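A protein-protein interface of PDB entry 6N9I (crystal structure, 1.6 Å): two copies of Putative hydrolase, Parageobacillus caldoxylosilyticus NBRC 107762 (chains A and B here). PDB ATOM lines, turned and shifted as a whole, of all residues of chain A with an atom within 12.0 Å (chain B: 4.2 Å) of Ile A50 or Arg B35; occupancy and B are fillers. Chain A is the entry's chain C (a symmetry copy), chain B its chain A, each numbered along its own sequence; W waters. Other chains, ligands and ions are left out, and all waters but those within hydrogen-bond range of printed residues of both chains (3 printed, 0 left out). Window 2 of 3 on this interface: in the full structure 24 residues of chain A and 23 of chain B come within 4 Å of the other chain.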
ATOM      1  N   MET A  44     -27.738  12.319  24.140  1.00  0.00           N
ATOM      2  CA  MET A  44     -27.085  13.406  23.407  1.00  0.00           C
ATOM      3  C   MET A  44     -27.352  14.750  24.093  1.00  0.00           C
ATOM      4  O   MET A  44     -27.726  15.723  23.438  1.00  0.00           O
ATOM      5  CB  MET A  44     -27.601  13.468  21.966  1.00  0.00           C
ATOM      6  CG  MET A  44     -27.384  12.185  21.189  1.00  0.00           C
ATOM      7  SD  MET A  44     -25.635  11.758  21.024  1.00  0.00           S
ATOM      8  CE  MET A  44     -24.991  13.270  20.311  1.00  0.00           C
ATOM      9  N   ASN A  46     -25.372  16.850  25.342  1.00  0.00           N
ATOM     10  CA  ASN A  46     -24.346  17.859  25.093  1.00  0.00           C
ATOM     11  C   ASN A  46     -23.519  17.472  23.870  1.00  0.00           C
ATOM     12  O   ASN A  46     -22.355  17.096  23.996  1.00  0.00           O
ATOM     13  CB  ASN A  46     -23.442  18.037  26.314  1.00  0.00           C
ATOM     14  CG  ASN A  46     -22.343  19.054  26.091  1.00  0.00           C
ATOM     15  OD1 ASN A  46     -22.520  20.007  25.336  1.00  0.00           O
ATOM     16  ND2 ASN A  46     -21.209  18.858  26.744  1.00  0.00           N
ATOM     17  N   PRO A  47     -24.086  17.558  22.647  1.00  0.00           N
ATOM     18  CA  PRO A  47     -23.361  17.158  21.442  1.00  0.00           C
ATOM     19  C   PRO A  47     -22.125  18.028  21.170  1.00  0.00           C
ATOM     20  O   PRO A  47     -22.148  19.248  21.386  1.00  0.00           O
ATOM     21  CB  PRO A  47     -24.386  17.330  20.310  1.00  0.00           C
ATOM     22  CG  PRO A  47     -25.731  17.381  21.007  1.00  0.00           C
ATOM     23  CD  PRO A  47     -25.454  18.010  22.356  1.00  0.00           C
ATOM     24  N   ALA A  48     -21.057  17.381  20.695  1.00  0.00           N
ATOM     25  CA  ALA A  48     -19.864  18.071  20.236  1.00  0.00           C
ATOM     26  C   ALA A  48     -20.212  18.907  18.999  1.00  0.00           C
ATOM     27  O   ALA A  48     -21.106  18.547  18.230  1.00  0.00           O
ATOM     28  CB  ALA A  48     -18.774  17.072  19.935  1.00  0.00           C
ATOM     29  N   THR A  49     -19.499  20.026  18.835  1.00  0.00           N
ATOM     30  CA  THR A  49     -19.644  20.910  17.685  1.00  0.00           C
ATOM     31  C   THR A  49     -18.245  21.248  17.158  1.00  0.00           C
ATOM     32  O   THR A  49     -17.242  20.820  17.734  1.00  0.00           O
ATOM     33  CB  THR A  49     -20.458  22.158  18.049  1.00  0.00           C
ATOM     34  OG1 THR A  49     -19.729  22.905  19.024  1.00  0.00           O
ATOM     35  CG2 THR A  49     -21.830  21.820  18.593  1.00  0.00           C
ATOM     36  N   ILE A  50     -18.181  22.015  16.065  1.00  0.00           N
ATOM     37  CA  ILE A  50     -16.925  22.234  15.349  1.00  0.00           C
ATOM     38  C   ILE A  50     -15.897  22.881  16.286  1.00  0.00           C
ATOM     39  O   ILE A  50     -14.713  22.556  16.231  1.00  0.00           O
ATOM     40  CB  ILE A  50     -17.135  23.068  14.069  1.00  0.00           C
ATOM     41  CG1 ILE A  50     -15.830  23.195  13.277  1.00  0.00           C
ATOM     42  CG2 ILE A  50     -17.736  24.428  14.390  1.00  0.00           C
ATOM     43  CD1 ILE A  50     -16.016  23.635  11.844  1.00  0.00           C
ATOM     44  N   HIS A  51     -16.354  23.790  17.151  1.00  0.00           N
ATOM     45  CA  HIS A  51     -15.449  24.547  18.017  1.00  0.00           C
ATOM     46  C   HIS A  51     -15.402  23.931  19.419  1.00  0.00           C
ATOM     47  O   HIS A  51     -14.752  24.466  20.315  1.00  0.00           O
ATOM     48  CB  HIS A  51     -15.842  26.027  18.040  1.00  0.00           C
ATOM     49  CG  HIS A  51     -15.755  26.679  16.701  1.00  0.00           C
ATOM     50  ND1 HIS A  51     -16.725  27.543  16.235  1.00  0.00           N
ATOM     51  CD2 HIS A  51     -14.832  26.577  15.721  1.00  0.00           C
ATOM     52  CE1 HIS A  51     -16.394  27.961  15.029  1.00  0.00           C
ATOM     53  NE2 HIS A  51     -15.237  27.381  14.690  1.00  0.00           N
ATOM     54  N   ASN A  52     -16.090  22.797  19.587  1.00  0.00           N
ATOM     55  CA  ASN A  52     -16.039  22.009  20.815  1.00  0.00           C
ATOM     56  C   ASN A  52     -16.117  20.531  20.445  1.00  0.00           C
ATOM     57  O   ASN A  52     -17.038  19.827  20.854  1.00  0.00           O
ATOM     58  CB  ASN A  52     -17.156  22.399  21.787  1.00  0.00           C
ATOM     59  CG  ASN A  52     -16.977  21.789  23.162  1.00  0.00           C
ATOM     60  OD1 ASN A  52     -15.853  21.594  23.618  1.00  0.00           O
ATOM     61  ND2 ASN A  52     -18.080  21.490  23.830  1.00  0.00           N
ATOM     62  N   PRO A  53     -15.137  20.028  19.662  1.00  0.00           N
ATOM     63  CA  PRO A  53     -15.240  18.712  19.029  1.00  0.00           C
ATOM     64  C   PRO A  53     -15.072  17.518  19.978  1.00  0.00           C
ATOM     65  O   PRO A  53     -15.466  16.401  19.639  1.00  0.00           O
ATOM     66  CB  PRO A  53     -14.083  18.735  18.018  1.00  0.00           C
ATOM     67  CG  PRO A  53     -13.054  19.635  18.667  1.00  0.00           C
ATOM     68  CD  PRO A  53     -13.875  20.712  19.344  1.00  0.00           C
ATOM     69  N   ASN A  54     -14.482  17.761  21.149  1.00  0.00           N
ATOM     70  CA  ASN A  54     -14.242  16.705  22.123  1.00  0.00           C
ATOM     71  C   ASN A  54     -15.082  16.973  23.377  1.00  0.00           C
ATOM     72  O   ASN A  54     -14.622  16.755  24.499  1.00  0.00           O
ATOM     73  CB  ASN A  54     -12.756  16.583  22.465  1.00  0.00           C
ATOM     74  CG  ASN A  54     -11.903  16.224  21.266  1.00  0.00           C
ATOM     75  OD1 ASN A  54     -12.244  15.328  20.495  1.00  0.00           O
ATOM     76  ND2 ASN A  54     -10.789  16.917  21.102  1.00  0.00           N
ATOM     77  N   ALA A  55     -16.313  17.449  23.165  1.00  0.00           N
ATOM     78  CA  ALA A  55     -17.246  17.719  24.255  1.00  0.00           C
ATOM     79  C   ALA A  55     -17.228  16.540  25.232  1.00  0.00           C
ATOM     80  O   ALA A  55     -17.222  15.384  24.816  1.00  0.00           O
ATOM     81  CB  ALA A  55     -18.632  17.957  23.706  1.00  0.00           C
ATOM     82  N   GLN A  56     -17.214  16.846  26.533  1.00  0.00           N
ATOM     83  CA  GLN A  56     -17.129  15.818  27.557  1.00  0.00           C
ATOM     84  C   GLN A  56     -18.482  15.707  28.267  1.00  0.00           C
ATOM     85  O   GLN A  56     -19.251  16.668  28.327  1.00  0.00           O
ATOM     86  CB  GLN A  56     -15.976  16.117  28.519  1.00  0.00           C
ATOM     87  CG  GLN A  56     -16.359  16.977  29.713  1.00  0.00           C
ATOM     88  CD  GLN A  56     -15.144  17.433  30.487  1.00  0.00           C
ATOM     89  OE1 GLN A  56     -14.180  17.944  29.923  1.00  0.00           O
ATOM     90  NE2 GLN A  56     -15.184  17.251  31.797  1.00  0.00           N
ATOM     91  N   MET B  34     -18.254  15.175   5.765  1.00  0.00           N
ATOM     92  CA  MET B  34     -18.977  15.780   6.867  1.00  0.00           C
ATOM     93  C   MET B  34     -18.341  15.305   8.176  1.00  0.00           C
ATOM     94  O   MET B  34     -17.749  14.226   8.232  1.00  0.00           O
ATOM     95  CB  MET B  34     -20.460  15.392   6.829  1.00  0.00           C
ATOM     96  CG  MET B  34     -21.281  15.963   7.973  1.00  0.00           C
ATOM     97  SD  MET B  34     -23.065  15.701   7.753  1.00  0.00           S
ATOM     98  CE  MET B  34     -23.392  16.837   6.406  1.00  0.00           C
ATOM     99  N   ARG B  35     -18.454  16.136   9.215  1.00  0.00           N
ATOM    100  CA  ARG B  35     -17.983  15.790  10.546  1.00  0.00           C
ATOM    101  C   ARG B  35     -19.130  15.970  11.542  1.00  0.00           C
ATOM    102  O   ARG B  35     -20.006  16.812  11.344  1.00  0.00           O
ATOM    103  CB  ARG B  35     -16.790  16.663  10.947  1.00  0.00           C
ATOM    104  CG  ARG B  35     -15.451  16.199  10.393  1.00  0.00           C
ATOM    105  CD  ARG B  35     -14.313  17.020  10.968  1.00  0.00           C
ATOM    106  NE  ARG B  35     -14.513  18.444  10.740  1.00  0.00           N
ATOM    107  CZ  ARG B  35     -14.004  19.407  11.499  1.00  0.00           C
ATOM    108  NH1 ARG B  35     -13.277  19.099  12.558  1.00  0.00           N
ATOM    109  NH2 ARG B  35     -14.228  20.674  11.197  1.00  0.00           N
ATOM    110  N   MET B  36     -19.111  15.168  12.610  1.00  0.00           N
ATOM    111  CA  MET B  36     -20.077  15.301  13.688  1.00  0.00           C
ATOM    112  C   MET B  36     -19.662  14.438  14.882  1.00  0.00           C
ATOM    113  O   MET B  36     -18.764  13.603  14.784  1.00  0.00           O
ATOM    114  CB  MET B  36     -21.474  14.877  13.227  1.00  0.00           C
ATOM    115  CG  MET B  36     -21.621  13.379  13.080  1.00  0.00           C
ATOM    116  SD  MET B  36     -23.209  12.913  12.361  1.00  0.00           S
ATOM    117  CE  MET B  36     -23.017  11.133  12.318  1.00  0.00           C
ATOM    118  N   PHE B  59     -14.990  14.204  17.208  1.00  0.00           N
ATOM    119  CA  PHE B  59     -15.592  14.737  16.003  1.00  0.00           C
ATOM    120  C   PHE B  59     -15.073  13.933  14.804  1.00  0.00           C
ATOM    121  O   PHE B  59     -13.971  14.180  14.331  1.00  0.00           O
ATOM    122  CB  PHE B  59     -15.235  16.219  15.877  1.00  0.00           C
ATOM    123  CG  PHE B  59     -16.339  17.112  15.375  1.00  0.00           C
ATOM    124  CD1 PHE B  59     -17.571  17.144  16.009  1.00  0.00           C
ATOM    125  CD2 PHE B  59     -16.133  17.948  14.290  1.00  0.00           C
ATOM    126  CE1 PHE B  59     -18.579  17.979  15.555  1.00  0.00           C
ATOM    127  CE2 PHE B  59     -17.143  18.780  13.836  1.00  0.00           C
ATOM    128  CZ  PHE B  59     -18.363  18.795  14.468  1.00  0.00           C
ATOM    129  N   VAL B  60     -15.864  12.963  14.333  1.00  0.00           N
ATOM    130  CA  VAL B  60     -15.400  12.031  13.300  1.00  0.00           C
ATOM    131  C   VAL B  60     -15.803  12.545  11.916  1.00  0.00           C
ATOM    132  O   VAL B  60     -16.827  13.210  11.753  1.00  0.00           O
ATOM    133  CB  VAL B  60     -15.931  10.603  13.525  1.00  0.00           C
ATOM    134  CG1 VAL B  60     -15.388  10.001  14.810  1.00  0.00           C
ATOM    135  CG2 VAL B  60     -17.451  10.557  13.501  1.00  0.00           C
ATOM    136  N   GLU B  61     -14.974  12.200  10.926  1.00  0.00           N
ATOM    137  CA  GLU B  61     -15.187  12.571   9.542  1.00  0.00           C
ATOM    138  C   GLU B  61     -15.673  11.345   8.765  1.00  0.00           C
ATOM    139  O   GLU B  61     -15.180  10.237   8.962  1.00  0.00           O
ATOM    140  CB  GLU B  61     -13.893  13.108   8.932  1.00  0.00           C
ATOM    141  CG  GLU B  61     -14.090  13.783   7.589  1.00  0.00           C
ATOM    142  CD  GLU B  61     -12.828  14.418   7.038  1.00  0.00           C
ATOM    143  OE1 GLU B  61     -11.827  13.694   6.895  1.00  0.00           O
ATOM    144  OE2 GLU B  61     -12.847  15.636   6.770  1.00  0.00           O
ATOM    145  N   GLN B  99     -22.383  24.042  12.552  1.00  0.00           N
ATOM    146  CA  GLN B  99     -21.359  23.809  13.564  1.00  0.00           C
ATOM    147  C   GLN B  99     -21.497  22.392  14.134  1.00  0.00           C
ATOM    148  O   GLN B  99     -20.544  21.854  14.700  1.00  0.00           O
ATOM    149  CB  GLN B  99     -21.435  24.880  14.657  1.00  0.00           C
ATOM    150  CG  GLN B  99     -21.138  26.282  14.139  1.00  0.00           C
ATOM    151  CD  GLN B  99     -20.787  27.266  15.231  1.00  0.00           C
ATOM    152  OE1 GLN B  99     -20.742  28.476  15.010  1.00  0.00           O
ATOM    153  NE2 GLN B  99     -20.526  26.757  16.423  1.00  0.00           N
ATOM    154  N   MET B 100     -22.676  21.787  13.967  1.00  0.00           N
ATOM    155  CA  MET B 100     -22.915  20.445  14.494  1.00  0.00           C
ATOM    156  C   MET B 100     -22.599  19.398  13.417  1.00  0.00           C
ATOM    157  O   MET B 100     -22.126  18.307  13.740  1.00  0.00           O
ATOM    158  CB  MET B 100     -24.359  20.277  14.979  1.00  0.00           C
ATOM    159  CG  MET B 100     -24.512  19.193  16.036  1.00  0.00           C
ATOM    160  SD  MET B 100     -26.006  19.372  17.048  1.00  0.00           S
ATOM    161  CE  MET B 100     -25.467  20.620  18.216  1.00  0.00           C
ATOM    162  N   PHE B 101     -22.843  19.742  12.147  1.00  0.00           N
ATOM    163  CA  PHE B 101     -22.630  18.812  11.034  1.00  0.00           C
ATOM    164  C   PHE B 101     -21.918  19.508   9.879  1.00  0.00           C
ATOM    165  O   PHE B 101     -22.400  19.487   8.749  1.00  0.00           O
ATOM    166  CB  PHE B 101     -23.965  18.243  10.551  1.00  0.00           C
ATOM    167  CG  PHE B 101     -24.827  17.658  11.641  1.00  0.00           C
ATOM    168  CD1 PHE B 101     -24.537  16.419  12.189  1.00  0.00           C
ATOM    169  CD2 PHE B 101     -25.929  18.349  12.117  1.00  0.00           C
ATOM    170  CE1 PHE B 101     -25.331  15.884  13.190  1.00  0.00           C
ATOM    171  CE2 PHE B 101     -26.723  17.813  13.119  1.00  0.00           C
ATOM    172  CZ  PHE B 101     -26.423  16.582  13.652  1.00  0.00           C
ATOM    173  N   PRO B 102     -20.735  20.117  10.113  1.00  0.00           N
ATOM    174  CA  PRO B 102     -20.046  20.869   9.067  1.00  0.00           C
ATOM    175  C   PRO B 102     -19.715  19.987   7.856  1.00  0.00           C
ATOM    176  O   PRO B 102     -19.190  18.884   8.010  1.00  0.00           O
ATOM    177  CB  PRO B 102     -18.766  21.375   9.751  1.00  0.00           C
ATOM    178  CG  PRO B 102     -18.570  20.430  10.919  1.00  0.00           C
ATOM    179  CD  PRO B 102     -19.971  20.071  11.368  1.00  0.00           C
HETATM  180  O   HOH W   1     -12.349  15.039  17.902  1.00  0.00           O
HETATM  181  O   HOH W   2     -19.037  25.158  17.887  1.00  0.00           O
HETATM  182  O   HOH W   3     -22.127  16.916  16.196  1.00  0.00           O
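The backbone NH (N) of Phe B59 is in hydrogen-bond range of the backbone carbonyl oxygen (O) of Pro A53 (3.3 Å).
N of Ile A50 lies within hydrogen-bond range of O of Gln B99 (2.7 Å).
N of Arg B35 lies within hydrogen-bond range of O of Pro B102 (3.1 Å).
CE1 of Phe B59 touches O of Ala A48, at 3.7 Å.
C of Thr A49 touches CZ of Phe B59, at 3.6 Å.
Thr A49 touches Gln B99 (CA to O, 3.3 Å).
Met B100 touches Thr A49.
NH2 of Arg B35 touches CD1 of Ile A50 (3.5 Å).
Phe B59 touches Ile A50 (CZ to N, 3.6 Å).
His A51 touches Gln B99.
Of the printed residues of chain B, Ala A48 touches Phe B59 (3.7 Å).
Of the printed residues of chain B, Ile A50 touches Arg B35 (3.5 Å), Phe B59 (3.6 Å) and Gln B99 (2.7 Å).
Of the printed residues of chain B, His A51 touches Gln B99 (3.9 Å).
Asn A52 touches none of the printed residues of chain B.
Printed residues of chain B within 4 Å of Pro A53: Phe B59.
Gln A56 touches none of the printed residues of chain B.
Of the printed residues of chain A, Arg B35 touches Ile A50 (3.5 Å).
No residue of chain A comes within 4 Å of Met B36.
Val B60 touches none of the printed residues of chain A.
No residue of chain A comes within 4 Å of Glu B61.
Gln B99 touches three residues of chain A.
No residue of chain A comes within 4 Å of Phe B101.
No residue of chain A comes within 4 Å of Pro B102.
The nearest printed residue of chain B that does not touch Ile A50 is Pro B102 (4.1 Å).
The nearest printed residue of chain B that does not touch Thr A49 is Pro B102 (6.2 Å).
Hydrophobic or aromatic side chains of chain B that line the printed part of chain A: Phe B59 and Met B100.
Of the 12 printed residues of chain A, 5 touch a printed residue of chain B.
No position is printed for both chains.
Of the 9 pairs that touch across the chains among the printed residues, none has its exchanged pair printed and touching as well.
Water W1 bridges OD1 of Asn A54 (2.6 Å) and N of Phe B59 (2.9 Å).
Water W2 lies within hydrogen-bond range of OG1 of Thr A49 (2.6 Å), NE2 of Gln B99 (2.6 Å) and N of His A51 (3.1 Å).
Water W3 lies within hydrogen-bond range of O of Ala A48 (2.8 Å) and O of Met B100 (2.8 Å).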
